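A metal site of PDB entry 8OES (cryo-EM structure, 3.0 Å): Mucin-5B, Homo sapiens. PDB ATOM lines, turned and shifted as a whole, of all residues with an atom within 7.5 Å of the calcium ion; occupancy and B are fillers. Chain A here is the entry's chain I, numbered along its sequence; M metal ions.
OE1 of Glu 27 lies within hydrogen-bond range of N of Gly 14, 3.4 Å away.
The backbone NH (N) of Leu 73 is in hydrogen-bond range of the backbone carbonyl oxygen (O) of Glu 27 (2.9 Å).
A ring nitrogen (NE2) of His 15 is in hydrogen-bond range of the backbone carbonyl oxygen (O) of Gly 24.
The calcium ion is bound by the side-chain carboxylate of Glu 27, the side-chain carboxylate of Asp 25, the side-chain amide oxygen of Asn 13, the backbone carbonyl oxygen of His 15 and the backbone carbonyl oxygen of Tyr 88.
The calcium ion has five donor atoms within binding distance.
Slightly farther from the calcium ion lies OD1 of Asp 25 (3.0 Å).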
ATOM      1  N   TYR A  12      31.698  -3.075  -5.404  1.00  0.00           N
ATOM      2  CA  TYR A  12      31.368  -1.963  -4.507  1.00  0.00           C
ATOM      3  C   TYR A  12      30.077  -2.283  -3.770  1.00  0.00           C
ATOM      4  O   TYR A  12      28.978  -2.129  -4.332  1.00  0.00           O
ATOM      5  CB  TYR A  12      31.252  -0.652  -5.280  1.00  0.00           C
ATOM      6  CG  TYR A  12      32.540  -0.189  -5.909  1.00  0.00           C
ATOM      7  CD1 TYR A  12      33.478   0.525  -5.159  1.00  0.00           C
ATOM      8  CD2 TYR A  12      32.828  -0.459  -7.240  1.00  0.00           C
ATOM      9  CE1 TYR A  12      34.656   0.950  -5.731  1.00  0.00           C
ATOM     10  CE2 TYR A  12      34.006  -0.034  -7.812  1.00  0.00           C
ATOM     11  CZ  TYR A  12      34.924   0.666  -7.056  1.00  0.00           C
ATOM     12  OH  TYR A  12      36.102   1.091  -7.627  1.00  0.00           O
ATOM     13  N   ASN A  13      30.183  -2.720  -2.515  1.00  0.00           N
ATOM     14  CA  ASN A  13      29.029  -2.985  -1.661  1.00  0.00           C
ATOM     15  C   ASN A  13      29.076  -1.997  -0.504  1.00  0.00           C
ATOM     16  O   ASN A  13      29.581  -2.293   0.574  1.00  0.00           O
ATOM     17  CB  ASN A  13      29.048  -4.431  -1.165  1.00  0.00           C
ATOM     18  CG  ASN A  13      27.778  -4.806  -0.419  1.00  0.00           C
ATOM     19  OD1 ASN A  13      26.873  -3.992  -0.263  1.00  0.00           O
ATOM     20  ND2 ASN A  13      27.712  -6.053   0.035  1.00  0.00           N
ATOM     21  N   GLY A  14      28.510  -0.808  -0.732  1.00  0.00           N
ATOM     22  CA  GLY A  14      28.556   0.280   0.224  1.00  0.00           C
ATOM     23  C   GLY A  14      27.389   0.371   1.181  1.00  0.00           C
ATOM     24  O   GLY A  14      27.300   1.347   1.935  1.00  0.00           O
ATOM     25  N   HIS A  15      26.489  -0.604   1.182  1.00  0.00           N
ATOM     26  CA  HIS A  15      25.302  -0.538   2.020  1.00  0.00           C
ATOM     27  C   HIS A  15      24.800  -1.953   2.280  1.00  0.00           C
ATOM     28  O   HIS A  15      25.058  -2.875   1.494  1.00  0.00           O
ATOM     29  CB  HIS A  15      24.206   0.304   1.359  1.00  0.00           C
ATOM     30  CG  HIS A  15      22.920   0.346   2.123  1.00  0.00           C
ATOM     31  ND1 HIS A  15      22.707   1.177   3.188  1.00  0.00           N
ATOM     32  CD2 HIS A  15      21.774  -0.358   1.959  1.00  0.00           C
ATOM     33  CE1 HIS A  15      21.481   0.994   3.658  1.00  0.00           C
ATOM     34  NE2 HIS A  15      20.893   0.067   2.925  1.00  0.00           N
ATOM     35  N   ARG A  16      24.081  -2.112   3.383  1.00  0.00           N
ATOM     36  CA  ARG A  16      23.409  -3.365   3.693  1.00  0.00           C
ATOM     37  C   ARG A  16      21.921  -3.102   3.787  1.00  0.00           C
ATOM     38  O   ARG A  16      21.490  -2.367   4.684  1.00  0.00           O
ATOM     39  CB  ARG A  16      23.940  -3.957   4.995  1.00  0.00           C
ATOM     40  CG  ARG A  16      25.368  -4.446   4.897  1.00  0.00           C
ATOM     41  CD  ARG A  16      25.533  -5.445   3.755  1.00  0.00           C
ATOM     42  NE  ARG A  16      26.717  -6.284   3.861  1.00  0.00           N
ATOM     43  CZ  ARG A  16      27.088  -6.988   4.926  1.00  0.00           C
ATOM     44  NH1 ARG A  16      26.327  -7.057   6.005  1.00  0.00           N
ATOM     45  NH2 ARG A  16      28.237  -7.657   4.898  1.00  0.00           N
ATOM     46  N   PRO A  17      21.111  -3.667   2.876  1.00  0.00           N
ATOM     47  CA  PRO A  17      19.695  -3.301   2.841  1.00  0.00           C
ATOM     48  C   PRO A  17      18.990  -3.604   4.151  1.00  0.00           C
ATOM     49  O   PRO A  17      19.303  -4.570   4.854  1.00  0.00           O
ATOM     50  CB  PRO A  17      19.141  -4.160   1.695  1.00  0.00           C
ATOM     51  CG  PRO A  17      20.180  -5.194   1.438  1.00  0.00           C
ATOM     52  CD  PRO A  17      21.479  -4.573   1.784  1.00  0.00           C
ATOM     53  N   GLY A  24      15.950  -1.179   1.777  1.00  0.00           N
ATOM     54  CA  GLY A  24      16.469  -1.685   0.535  1.00  0.00           C
ATOM     55  C   GLY A  24      17.889  -1.218   0.329  1.00  0.00           C
ATOM     56  O   GLY A  24      18.514  -0.674   1.233  1.00  0.00           O
ATOM     57  N   ASP A  25      18.385  -1.420  -0.878  1.00  0.00           N
ATOM     58  CA  ASP A  25      19.746  -1.035  -1.229  1.00  0.00           C
ATOM     59  C   ASP A  25      19.699   0.088  -2.248  1.00  0.00           C
ATOM     60  O   ASP A  25      18.983  -0.007  -3.246  1.00  0.00           O
ATOM     61  CB  ASP A  25      20.542  -2.217  -1.789  1.00  0.00           C
ATOM     62  CG  ASP A  25      22.041  -2.030  -1.617  1.00  0.00           C
ATOM     63  OD1 ASP A  25      22.446  -0.996  -1.052  1.00  0.00           O
ATOM     64  OD2 ASP A  25      22.814  -2.921  -2.041  1.00  0.00           O
ATOM     65  N   PHE A  26      20.456   1.156  -1.992  1.00  0.00           N
ATOM     66  CA  PHE A  26      20.471   2.339  -2.858  1.00  0.00           C
ATOM     67  C   PHE A  26      21.933   2.675  -3.136  1.00  0.00           C
ATOM     68  O   PHE A  26      22.518   3.512  -2.454  1.00  0.00           O
ATOM     69  CB  PHE A  26      19.720   3.489  -2.196  1.00  0.00           C
ATOM     70  CG  PHE A  26      18.486   3.052  -1.446  1.00  0.00           C
ATOM     71  CD1 PHE A  26      17.282   2.884  -2.111  1.00  0.00           C
ATOM     72  CD2 PHE A  26      18.525   2.827  -0.081  1.00  0.00           C
ATOM     73  CE1 PHE A  26      16.151   2.487  -1.425  1.00  0.00           C
ATOM     74  CE2 PHE A  26      17.394   2.430   0.605  1.00  0.00           C
ATOM     75  CZ  PHE A  26      16.209   2.266  -0.069  1.00  0.00           C
ATOM     76  N   GLU A  27      22.511   2.022  -4.150  1.00  0.00           N
ATOM     77  CA  GLU A  27      23.922   2.173  -4.487  1.00  0.00           C
ATOM     78  C   GLU A  27      24.017   3.145  -5.654  1.00  0.00           C
ATOM     79  O   GLU A  27      23.897   2.744  -6.811  1.00  0.00           O
ATOM     80  CB  GLU A  27      24.541   0.824  -4.840  1.00  0.00           C
ATOM     81  CG  GLU A  27      24.461  -0.237  -3.750  1.00  0.00           C
ATOM     82  CD  GLU A  27      25.371   0.046  -2.579  1.00  0.00           C
ATOM     83  OE1 GLU A  27      26.314   0.853  -2.732  1.00  0.00           O
ATOM     84  OE2 GLU A  27      25.173  -0.571  -1.514  1.00  0.00           O
ATOM     85  N   ALA A  51      25.375  -9.693  -3.843  1.00  0.00           N
ATOM     86  CA  ALA A  51      26.650  -9.970  -3.191  1.00  0.00           C
ATOM     87  C   ALA A  51      26.659 -11.337  -2.525  1.00  0.00           C
ATOM     88  O   ALA A  51      27.674 -12.044  -2.566  1.00  0.00           O
ATOM     89  CB  ALA A  51      26.967  -8.872  -2.178  1.00  0.00           C
ATOM     90  N   LEU A  73      22.502   1.328  -8.928  1.00  0.00           N
ATOM     91  CA  LEU A  73      21.627   0.206  -8.579  1.00  0.00           C
ATOM     92  C   LEU A  73      20.652   0.629  -7.501  1.00  0.00           C
ATOM     93  O   LEU A  73      21.021   1.329  -6.550  1.00  0.00           O
ATOM     94  CB  LEU A  73      22.465  -0.997  -8.129  1.00  0.00           C
ATOM     95  CG  LEU A  73      21.931  -2.353  -7.672  1.00  0.00           C
ATOM     96  CD1 LEU A  73      23.128  -3.264  -7.478  1.00  0.00           C
ATOM     97  CD2 LEU A  73      21.135  -2.317  -6.380  1.00  0.00           C
ATOM     98  N   HIS A  86      17.610  -8.213  -1.447  1.00  0.00           N
ATOM     99  CA  HIS A  86      18.864  -8.888  -1.155  1.00  0.00           C
ATOM    100  C   HIS A  86      19.972  -7.845  -1.033  1.00  0.00           C
ATOM    101  O   HIS A  86      19.757  -6.651  -1.263  1.00  0.00           O
ATOM    102  CB  HIS A  86      19.166  -9.913  -2.253  1.00  0.00           C
ATOM    103  CG  HIS A  86      18.071 -10.908  -2.453  1.00  0.00           C
ATOM    104  ND1 HIS A  86      17.553 -11.199  -3.706  1.00  0.00           N
ATOM    105  CD2 HIS A  86      17.387 -11.686  -1.580  1.00  0.00           C
ATOM    106  CE1 HIS A  86      16.612 -12.113  -3.580  1.00  0.00           C
ATOM    107  NE2 HIS A  86      16.491 -12.425  -2.307  1.00  0.00           N
ATOM    108  N   ASP A  87      21.167  -8.289  -0.656  1.00  0.00           N
ATOM    109  CA  ASP A  87      22.307  -7.384  -0.523  1.00  0.00           C
ATOM    110  C   ASP A  87      23.075  -7.383  -1.837  1.00  0.00           C
ATOM    111  O   ASP A  87      23.804  -8.328  -2.142  1.00  0.00           O
ATOM    112  CB  ASP A  87      23.197  -7.810   0.646  1.00  0.00           C
ATOM    113  CG  ASP A  87      22.440  -7.915   1.953  1.00  0.00           C
ATOM    114  OD1 ASP A  87      21.217  -8.170   1.918  1.00  0.00           O
ATOM    115  OD2 ASP A  87      23.057  -7.745   3.023  1.00  0.00           O
ATOM    116  N   TYR A  88      22.928  -6.309  -2.606  1.00  0.00           N
ATOM    117  CA  TYR A  88      23.512  -6.220  -3.936  1.00  0.00           C
ATOM    118  C   TYR A  88      24.820  -5.442  -3.895  1.00  0.00           C
ATOM    119  O   TYR A  88      25.153  -4.774  -2.918  1.00  0.00           O
ATOM    120  CB  TYR A  88      22.545  -5.544  -4.921  1.00  0.00           C
ATOM    121  CG  TYR A  88      21.219  -6.231  -5.141  1.00  0.00           C
ATOM    122  CD1 TYR A  88      20.231  -6.196  -4.172  1.00  0.00           C
ATOM    123  CD2 TYR A  88      20.943  -6.885  -6.333  1.00  0.00           C
ATOM    124  CE1 TYR A  88      19.014  -6.808  -4.370  1.00  0.00           C
ATOM    125  CE2 TYR A  88      19.725  -7.503  -6.547  1.00  0.00           C
ATOM    126  CZ  TYR A  88      18.769  -7.463  -5.552  1.00  0.00           C
ATOM    127  OH  TYR A  88      17.551  -8.067  -5.747  1.00  0.00           O
ATOM    128  N   GLU A  89      25.561  -5.543  -5.003  1.00  0.00           N
ATOM    129  CA  GLU A  89      26.699  -4.668  -5.256  1.00  0.00           C
ATOM    130  C   GLU A  89      26.871  -4.567  -6.771  1.00  0.00           C
ATOM    131  O   GLU A  89      26.144  -5.197  -7.536  1.00  0.00           O
ATOM    132  CB  GLU A  89      27.982  -5.168  -4.566  1.00  0.00           C
ATOM    133  CG  GLU A  89      28.919  -6.111  -5.334  1.00  0.00           C
ATOM    134  CD  GLU A  89      28.247  -7.254  -6.072  1.00  0.00           C
ATOM    135  OE1 GLU A  89      28.948  -7.921  -6.862  1.00  0.00           O
ATOM    136  OE2 GLU A  89      27.063  -7.549  -5.825  1.00  0.00           O
ATOM    137  N   LEU A  90      27.837  -3.751  -7.196  1.00  0.00           N
ATOM    138  CA  LEU A  90      28.016  -3.473  -8.609  1.00  0.00           C
ATOM    139  C   LEU A  90      29.467  -3.098  -8.880  1.00  0.00           C
ATOM    140  O   LEU A  90      30.228  -2.792  -7.963  1.00  0.00           O
ATOM    141  CB  LEU A  90      27.075  -2.361  -9.095  1.00  0.00           C
ATOM    142  CG  LEU A  90      27.083  -1.029  -8.339  1.00  0.00           C
ATOM    143  CD1 LEU A  90      26.504   0.070  -9.211  1.00  0.00           C
ATOM    144  CD2 LEU A  90      26.278  -1.134  -7.069  1.00  0.00           C
HETATM  145 CA    CA M   1      24.869  -2.795  -0.978  1.00  0.00          CA
